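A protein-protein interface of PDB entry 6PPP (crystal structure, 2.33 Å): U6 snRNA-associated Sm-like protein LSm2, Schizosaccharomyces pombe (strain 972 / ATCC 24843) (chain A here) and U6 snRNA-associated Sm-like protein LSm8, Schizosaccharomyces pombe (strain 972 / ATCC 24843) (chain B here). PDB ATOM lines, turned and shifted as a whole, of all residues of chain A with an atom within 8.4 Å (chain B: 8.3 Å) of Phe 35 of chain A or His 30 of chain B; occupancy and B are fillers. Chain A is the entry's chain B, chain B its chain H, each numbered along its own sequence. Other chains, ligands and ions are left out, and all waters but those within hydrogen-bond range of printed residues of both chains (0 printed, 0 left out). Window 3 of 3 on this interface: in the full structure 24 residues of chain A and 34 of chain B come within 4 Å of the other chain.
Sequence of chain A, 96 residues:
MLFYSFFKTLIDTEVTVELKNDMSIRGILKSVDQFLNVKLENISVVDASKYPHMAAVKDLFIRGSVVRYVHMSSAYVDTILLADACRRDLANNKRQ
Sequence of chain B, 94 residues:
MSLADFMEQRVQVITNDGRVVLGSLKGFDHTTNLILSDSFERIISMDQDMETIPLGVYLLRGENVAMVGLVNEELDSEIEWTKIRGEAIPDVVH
NH1 of Arg 63 of chain A sits at hydrogen-bond distance from O of Thr 31 of chain B (3.0 Å).
NE of Arg 63 of chain A sits at hydrogen-bond distance from OG1 of Thr 32 of chain B (2.7 Å).
NE of Arg 63 of chain A is in hydrogen-bond range of O of Gly 62 of chain B, 2.9 Å away.
OD1 of Asp 33 of chain A lies within hydrogen-bond range of N of Phe 35 of chain A, 3.0 Å away.
The guanidinium group (NH2) of Arg 63 of chain A is in hydrogen-bond range of the side-chain hydroxyl (OG) of Ser 65 of chain A (2.6 Å).
OD1 of Asp 29 of chain B sits at hydrogen-bond distance from OG1 of Thr 31 of chain B, 3.2 Å away.
The side-chain hydroxyl (OG1) of Thr 31 of chain B is in hydrogen-bond range of the side-chain amide nitrogen (ND2) of Asn 33 of chain B.
The side-chain amide oxygen of Asn 33 of chain B sits at hydrogen-bond distance from the backbone NH of Gly 62 of chain B, at 2.7 Å.
Among the printed residues, merely in contact across the chains: Phe 35 of chain A with His 30 of chain B (3.5 Å), Phe 61 of chain A with Leu 3 of chain B (3.9 Å) and Phe 61 of chain A with Thr 32 of chain B (3.5 Å).
Tyr 4 of chain A touches none of the printed residues of chain B.
Of chain B, only His 30 comes within 4 Å of Phe 35 of chain A.
Gly 64 of chain A touches none of the printed residues of chain B.
His 30 of chain B touches just one residue of chain A: Phe 35 (3.5 Å).
Of the printed residues of chain A, Thr 32 of chain B touches Phe 61 (3.5 Å) and Arg 63 (2.7 Å).
Of the printed residues of chain A, Gly 62 of chain B touches Arg 63.
The nearest residue of chain A that does not touch His 30 of chain B is Asn 37 of chain A (5.5 Å).
The nearest printed residue of chain B that does not touch Phe 61 of chain A is Met 1 of chain B (4.8 Å).
Of the 17 printed residues of chain A, 3 touch a printed residue of chain B.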
ATOM      1  N   MET A   1       5.611  19.255  31.547  1.00  0.00           N
ATOM      2  CA  MET A   1       4.482  18.341  31.602  1.00  0.00           C
ATOM      3  C   MET A   1       3.950  18.170  33.034  1.00  0.00           C
ATOM      4  O   MET A   1       2.919  17.527  33.241  1.00  0.00           O
ATOM      5  CB  MET A   1       4.798  17.034  30.903  1.00  0.00           C
ATOM      6  CG  MET A   1       4.280  17.181  29.456  1.00  0.00           C
ATOM      7  SD  MET A   1       3.962  15.747  28.388  1.00  0.00           S
ATOM      8  CE  MET A   1       3.419  14.495  29.554  1.00  0.00           C
ATOM      9  N   TYR A   4       0.429  20.011  33.667  1.00  0.00           N
ATOM     10  CA  TYR A   4      -0.491  19.294  32.795  1.00  0.00           C
ATOM     11  C   TYR A   4      -0.831  17.899  33.340  1.00  0.00           C
ATOM     12  O   TYR A   4      -2.006  17.508  33.366  1.00  0.00           O
ATOM     13  CB  TYR A   4       0.108  19.180  31.393  1.00  0.00           C
ATOM     14  CG  TYR A   4      -0.497  18.126  30.538  1.00  0.00           C
ATOM     15  CD1 TYR A   4      -1.727  18.310  29.907  1.00  0.00           C
ATOM     16  CD2 TYR A   4       0.178  16.948  30.293  1.00  0.00           C
ATOM     17  CE1 TYR A   4      -2.286  17.265  29.056  1.00  0.00           C
ATOM     18  CE2 TYR A   4      -0.362  15.937  29.471  1.00  0.00           C
ATOM     19  CZ  TYR A   4      -1.601  16.095  28.875  1.00  0.00           C
ATOM     20  OH  TYR A   4      -2.085  15.035  28.088  1.00  0.00           O
ATOM     21  N   PHE A   7      -3.085  18.420  36.380  1.00  0.00           N
ATOM     22  CA  PHE A   7      -4.436  18.813  36.001  1.00  0.00           C
ATOM     23  C   PHE A   7      -5.159  17.637  35.416  1.00  0.00           C
ATOM     24  O   PHE A   7      -6.380  17.513  35.576  1.00  0.00           O
ATOM     25  CB  PHE A   7      -4.410  19.968  35.015  1.00  0.00           C
ATOM     26  CG  PHE A   7      -4.265  21.308  35.692  1.00  0.00           C
ATOM     27  CD1 PHE A   7      -5.094  21.655  36.718  1.00  0.00           C
ATOM     28  CD2 PHE A   7      -3.324  22.205  35.300  1.00  0.00           C
ATOM     29  CE1 PHE A   7      -4.998  22.863  37.349  1.00  0.00           C
ATOM     30  CE2 PHE A   7      -3.224  23.421  35.916  1.00  0.00           C
ATOM     31  CZ  PHE A   7      -4.064  23.758  36.949  1.00  0.00           C
ATOM     32  N   VAL A  32      -7.703  19.124  29.877  1.00  0.00           N
ATOM     33  CA  VAL A  32      -6.594  20.071  30.028  1.00  0.00           C
ATOM     34  C   VAL A  32      -5.569  19.660  28.981  1.00  0.00           C
ATOM     35  O   VAL A  32      -5.498  18.490  28.602  1.00  0.00           O
ATOM     36  CB  VAL A  32      -5.969  20.049  31.440  1.00  0.00           C
ATOM     37  CG1 VAL A  32      -5.147  18.827  31.627  1.00  0.00           C
ATOM     38  CG2 VAL A  32      -5.085  21.315  31.660  1.00  0.00           C
ATOM     39  N   ASP A  33      -4.838  20.622  28.420  1.00  0.00           N
ATOM     40  CA  ASP A  33      -3.819  20.172  27.460  1.00  0.00           C
ATOM     41  C   ASP A  33      -2.419  20.711  27.703  1.00  0.00           C
ATOM     42  O   ASP A  33      -2.171  21.386  28.700  1.00  0.00           O
ATOM     43  CB  ASP A  33      -4.239  20.450  26.035  1.00  0.00           C
ATOM     44  CG  ASP A  33      -4.416  21.901  25.767  1.00  0.00           C
ATOM     45  OD1 ASP A  33      -3.715  22.735  26.418  1.00  0.00           O
ATOM     46  OD2 ASP A  33      -5.286  22.199  24.899  1.00  0.00           O
ATOM     47  N   GLN A  34      -1.522  20.461  26.751  1.00  0.00           N
ATOM     48  CA  GLN A  34      -0.122  20.784  26.971  1.00  0.00           C
ATOM     49  C   GLN A  34       0.088  22.259  27.210  1.00  0.00           C
ATOM     50  O   GLN A  34       1.006  22.617  27.959  1.00  0.00           O
ATOM     51  CB  GLN A  34       0.682  20.335  25.736  1.00  0.00           C
ATOM     52  CG  GLN A  34       2.183  20.356  25.904  1.00  0.00           C
ATOM     53  CD  GLN A  34       2.685  19.339  26.935  1.00  0.00           C
ATOM     54  OE1 GLN A  34       2.526  18.120  26.759  1.00  0.00           O
ATOM     55  NE2 GLN A  34       3.288  19.842  28.024  1.00  0.00           N
ATOM     56  N   PHE A  35      -0.765  23.128  26.631  1.00  0.00           N
ATOM     57  CA  PHE A  35      -0.711  24.581  26.835  1.00  0.00           C
ATOM     58  C   PHE A  35      -1.420  24.986  28.112  1.00  0.00           C
ATOM     59  O   PHE A  35      -1.451  26.195  28.445  1.00  0.00           O
ATOM     60  CB  PHE A  35      -1.339  25.373  25.669  1.00  0.00           C
ATOM     61  CG  PHE A  35      -0.832  24.972  24.274  1.00  0.00           C
ATOM     62  CD1 PHE A  35       0.498  25.229  23.894  1.00  0.00           C
ATOM     63  CD2 PHE A  35      -1.693  24.374  23.350  1.00  0.00           C
ATOM     64  CE1 PHE A  35       0.969  24.872  22.651  1.00  0.00           C
ATOM     65  CE2 PHE A  35      -1.223  23.991  22.086  1.00  0.00           C
ATOM     66  CZ  PHE A  35       0.107  24.248  21.730  1.00  0.00           C
ATOM     67  N   LEU A  36      -1.993  24.007  28.833  1.00  0.00           N
ATOM     68  CA  LEU A  36      -2.895  24.267  29.958  1.00  0.00           C
ATOM     69  C   LEU A  36      -4.186  24.991  29.515  1.00  0.00           C
ATOM     70  O   LEU A  36      -4.865  25.588  30.330  1.00  0.00           O
ATOM     71  CB  LEU A  36      -2.182  25.053  31.067  1.00  0.00           C
ATOM     72  CG  LEU A  36      -0.868  24.372  31.483  1.00  0.00           C
ATOM     73  CD1 LEU A  36      -0.188  25.061  32.646  1.00  0.00           C
ATOM     74  CD2 LEU A  36      -1.161  22.945  31.912  1.00  0.00           C
ATOM     75  N   ASN A  37      -4.577  24.932  28.231  1.00  0.00           N
ATOM     76  CA  ASN A  37      -5.988  25.164  27.894  1.00  0.00           C
ATOM     77  C   ASN A  37      -6.860  24.251  28.750  1.00  0.00           C
ATOM     78  O   ASN A  37      -6.459  23.146  29.122  1.00  0.00           O
ATOM     79  CB  ASN A  37      -6.310  24.783  26.426  1.00  0.00           C
ATOM     80  CG  ASN A  37      -5.620  25.658  25.399  1.00  0.00           C
ATOM     81  OD1 ASN A  37      -5.574  26.886  25.522  1.00  0.00           O
ATOM     82  ND2 ASN A  37      -5.047  25.020  24.390  1.00  0.00           N
ATOM     83  N   VAL A  38      -8.025  24.711  29.143  1.00  0.00           N
ATOM     84  CA  VAL A  38      -8.799  23.914  30.084  1.00  0.00           C
ATOM     85  C   VAL A  38     -10.276  23.879  29.655  1.00  0.00           C
ATOM     86  O   VAL A  38     -10.862  24.911  29.296  1.00  0.00           O
ATOM     87  CB  VAL A  38      -8.581  24.532  31.474  1.00  0.00           C
ATOM     88  CG1 VAL A  38      -9.452  25.736  31.626  1.00  0.00           C
ATOM     89  CG2 VAL A  38      -8.841  23.561  32.537  1.00  0.00           C
ATOM     90  N   PHE A  61     -14.759  26.313  27.237  1.00  0.00           N
ATOM     91  CA  PHE A  61     -13.314  26.282  27.035  1.00  0.00           C
ATOM     92  C   PHE A  61     -12.692  27.587  27.498  1.00  0.00           C
ATOM     93  O   PHE A  61     -13.195  28.657  27.151  1.00  0.00           O
ATOM     94  CB  PHE A  61     -13.032  26.030  25.555  1.00  0.00           C
ATOM     95  CG  PHE A  61     -11.591  26.215  25.130  1.00  0.00           C
ATOM     96  CD1 PHE A  61     -11.015  27.480  25.010  1.00  0.00           C
ATOM     97  CD2 PHE A  61     -10.846  25.125  24.746  1.00  0.00           C
ATOM     98  CE1 PHE A  61      -9.703  27.627  24.568  1.00  0.00           C
ATOM     99  CE2 PHE A  61      -9.530  25.268  24.304  1.00  0.00           C
ATOM    100  CZ  PHE A  61      -8.961  26.496  24.202  1.00  0.00           C
ATOM    101  N   ILE A  62     -11.620  27.502  28.295  1.00  0.00           N
ATOM    102  CA  ILE A  62     -10.870  28.662  28.789  1.00  0.00           C
ATOM    103  C   ILE A  62      -9.454  28.524  28.257  1.00  0.00           C
ATOM    104  O   ILE A  62      -8.813  27.485  28.473  1.00  0.00           O
ATOM    105  CB  ILE A  62     -10.852  28.725  30.318  1.00  0.00           C
ATOM    106  CG1 ILE A  62     -12.278  28.495  30.876  1.00  0.00           C
ATOM    107  CG2 ILE A  62     -10.175  30.035  30.774  1.00  0.00           C
ATOM    108  CD1 ILE A  62     -12.375  28.828  32.376  1.00  0.00           C
ATOM    109  N   ARG A  63      -8.945  29.576  27.619  1.00  0.00           N
ATOM    110  CA  ARG A  63      -7.596  29.526  27.045  1.00  0.00           C
ATOM    111  C   ARG A  63      -6.530  29.591  28.134  1.00  0.00           C
ATOM    112  O   ARG A  63      -6.673  30.317  29.117  1.00  0.00           O
ATOM    113  CB  ARG A  63      -7.386  30.680  26.072  1.00  0.00           C
ATOM    114  CG  ARG A  63      -6.245  30.491  25.062  1.00  0.00           C
ATOM    115  CD  ARG A  63      -6.035  31.813  24.298  1.00  0.00           C
ATOM    116  NE  ARG A  63      -5.290  31.689  23.046  1.00  0.00           N
ATOM    117  CZ  ARG A  63      -4.095  32.240  22.854  1.00  0.00           C
ATOM    118  NH1 ARG A  63      -3.477  32.105  21.681  1.00  0.00           N
ATOM    119  NH2 ARG A  63      -3.511  32.924  23.847  1.00  0.00           N
ATOM    120  N   GLY A  64      -5.481  28.772  28.002  1.00  0.00           N
ATOM    121  CA  GLY A  64      -4.534  28.701  29.104  1.00  0.00           C
ATOM    122  C   GLY A  64      -3.853  30.017  29.449  1.00  0.00           C
ATOM    123  O   GLY A  64      -3.513  30.248  30.614  1.00  0.00           O
ATOM    124  N   SER A  65      -3.637  30.900  28.462  1.00  0.00           N
ATOM    125  CA  SER A  65      -2.903  32.158  28.691  1.00  0.00           C
ATOM    126  C   SER A  65      -3.702  33.178  29.499  1.00  0.00           C
ATOM    127  O   SER A  65      -3.155  34.229  29.872  1.00  0.00           O
ATOM    128  CB  SER A  65      -2.517  32.799  27.367  1.00  0.00           C
ATOM    129  OG  SER A  65      -3.608  32.767  26.447  1.00  0.00           O
ATOM    130  N   VAL A  66      -5.012  32.967  29.648  1.00  0.00           N
ATOM    131  CA  VAL A  66      -5.861  33.909  30.348  1.00  0.00           C
ATOM    132  C   VAL A  66      -6.153  33.476  31.796  1.00  0.00           C
ATOM    133  O   VAL A  66      -6.793  34.248  32.542  1.00  0.00           O
ATOM    134  CB  VAL A  66      -7.164  34.059  29.548  1.00  0.00           C
ATOM    135  CG1 VAL A  66      -8.118  32.949  29.945  1.00  0.00           C
ATOM    136  CG2 VAL A  66      -7.785  35.362  29.756  1.00  0.00           C
ATOM    137  N   VAL A  67      -5.687  32.281  32.231  1.00  0.00           N
ATOM    138  CA  VAL A  67      -5.824  31.898  33.650  1.00  0.00           C
ATOM    139  C   VAL A  67      -4.854  32.679  34.547  1.00  0.00           C
ATOM    140  O   VAL A  67      -3.656  32.790  34.257  1.00  0.00           O
ATOM    141  CB  VAL A  67      -5.704  30.386  33.843  1.00  0.00           C
ATOM    142  CG1 VAL A  67      -6.771  29.696  33.010  1.00  0.00           C
ATOM    143  CG2 VAL A  67      -4.311  29.877  33.495  1.00  0.00           C
ATOM    144  N   MET B   1      -8.143  19.864  19.694  1.00  0.00           N
ATOM    145  CA  MET B   1      -8.327  20.446  21.024  1.00  0.00           C
ATOM    146  C   MET B   1      -9.655  20.020  21.633  1.00  0.00           C
ATOM    147  O   MET B   1     -10.486  19.378  20.975  1.00  0.00           O
ATOM    148  CB  MET B   1      -8.261  21.987  20.972  1.00  0.00           C
ATOM    149  N   LEU B   3     -11.750  21.909  21.826  1.00  0.00           N
ATOM    150  CA  LEU B   3     -12.579  22.606  20.858  1.00  0.00           C
ATOM    151  C   LEU B   3     -13.120  21.696  19.770  1.00  0.00           C
ATOM    152  O   LEU B   3     -14.157  22.012  19.177  1.00  0.00           O
ATOM    153  CB  LEU B   3     -11.752  23.703  20.184  1.00  0.00           C
ATOM    154  CG  LEU B   3     -11.745  25.001  20.972  1.00  0.00           C
ATOM    155  CD1 LEU B   3     -10.835  26.107  20.379  1.00  0.00           C
ATOM    156  CD2 LEU B   3     -13.187  25.453  21.075  1.00  0.00           C
ATOM    157  N   PHE B  28     -10.771  25.513  13.988  1.00  0.00           N
ATOM    158  CA  PHE B  28      -9.836  26.122  14.924  1.00  0.00           C
ATOM    159  C   PHE B  28      -8.460  25.522  14.666  1.00  0.00           C
ATOM    160  O   PHE B  28      -8.326  24.555  13.914  1.00  0.00           O
ATOM    161  CB  PHE B  28     -10.255  25.872  16.380  1.00  0.00           C
ATOM    162  CG  PHE B  28     -10.198  24.407  16.784  1.00  0.00           C
ATOM    163  CD1 PHE B  28     -11.312  23.585  16.626  1.00  0.00           C
ATOM    164  CD2 PHE B  28      -9.030  23.848  17.290  1.00  0.00           C
ATOM    165  CE1 PHE B  28     -11.277  22.243  16.977  1.00  0.00           C
ATOM    166  CE2 PHE B  28      -8.987  22.490  17.652  1.00  0.00           C
ATOM    167  CZ  PHE B  28     -10.110  21.689  17.492  1.00  0.00           C
ATOM    168  N   ASP B  29      -7.427  26.093  15.296  1.00  0.00           N
ATOM    169  CA  ASP B  29      -6.098  25.492  15.259  1.00  0.00           C
ATOM    170  C   ASP B  29      -5.450  25.638  16.622  1.00  0.00           C
ATOM    171  O   ASP B  29      -6.027  26.234  17.530  1.00  0.00           O
ATOM    172  CB  ASP B  29      -5.225  26.115  14.168  1.00  0.00           C
ATOM    173  CG  ASP B  29      -5.254  27.598  14.199  1.00  0.00           C
ATOM    174  OD1 ASP B  29      -5.224  28.174  15.311  1.00  0.00           O
ATOM    175  OD2 ASP B  29      -5.331  28.195  13.104  1.00  0.00           O
ATOM    176  N   HIS B  30      -4.189  25.178  16.717  1.00  0.00           N
ATOM    177  CA  HIS B  30      -3.444  25.037  17.972  1.00  0.00           C
ATOM    178  C   HIS B  30      -3.093  26.350  18.643  1.00  0.00           C
ATOM    179  O   HIS B  30      -2.497  26.307  19.722  1.00  0.00           O
ATOM    180  CB  HIS B  30      -2.136  24.267  17.748  1.00  0.00           C
ATOM    181  CG  HIS B  30      -1.140  25.004  16.901  1.00  0.00           C
ATOM    182  ND1 HIS B  30      -1.157  24.953  15.521  1.00  0.00           N
ATOM    183  CD2 HIS B  30      -0.111  25.823  17.232  1.00  0.00           C
ATOM    184  CE1 HIS B  30      -0.183  25.707  15.040  1.00  0.00           C
ATOM    185  NE2 HIS B  30       0.467  26.246  16.057  1.00  0.00           N
ATOM    186  N   THR B  31      -3.338  27.498  18.018  1.00  0.00           N
ATOM    187  CA  THR B  31      -3.213  28.760  18.730  1.00  0.00           C
ATOM    188  C   THR B  31      -4.570  29.316  19.133  1.00  0.00           C
ATOM    189  O   THR B  31      -4.659  30.496  19.502  1.00  0.00           O
ATOM    190  CB  THR B  31      -2.402  29.777  17.918  1.00  0.00           C
ATOM    191  OG1 THR B  31      -3.011  30.022  16.646  1.00  0.00           O
ATOM    192  CG2 THR B  31      -1.004  29.219  17.711  1.00  0.00           C
ATOM    193  N   THR B  32      -5.644  28.563  18.872  1.00  0.00           N
ATOM    194  CA  THR B  32      -7.046  28.926  19.132  1.00  0.00           C
ATOM    195  C   THR B  32      -7.606  29.986  18.179  1.00  0.00           C
ATOM    196  O   THR B  32      -8.604  30.630  18.516  1.00  0.00           O
ATOM    197  CB  THR B  32      -7.362  29.294  20.600  1.00  0.00           C
ATOM    198  OG1 THR B  32      -6.318  30.063  21.197  1.00  0.00           O
ATOM    199  CG2 THR B  32      -7.549  28.038  21.413  1.00  0.00           C
ATOM    200  N   ASN B  33      -6.971  30.278  17.039  1.00  0.00           N
ATOM    201  CA  ASN B  33      -7.712  30.964  15.968  1.00  0.00           C
ATOM    202  C   ASN B  33      -9.027  30.240  15.681  1.00  0.00           C
ATOM    203  O   ASN B  33      -9.070  29.008  15.654  1.00  0.00           O
ATOM    204  CB  ASN B  33      -6.905  30.983  14.662  1.00  0.00           C
ATOM    205  CG  ASN B  33      -5.542  31.590  14.816  1.00  0.00           C
ATOM    206  OD1 ASN B  33      -5.352  32.532  15.595  1.00  0.00           O
ATOM    207  ND2 ASN B  33      -4.571  31.050  14.075  1.00  0.00           N
ATOM    208  N   GLY B  62      -6.153  33.783  17.891  1.00  0.00           N
ATOM    209  CA  GLY B  62      -6.177  33.125  19.188  1.00  0.00           C
ATOM    210  C   GLY B  62      -5.650  33.980  20.334  1.00  0.00           C
ATOM    211  O   GLY B  62      -6.174  33.915  21.457  1.00  0.00           O
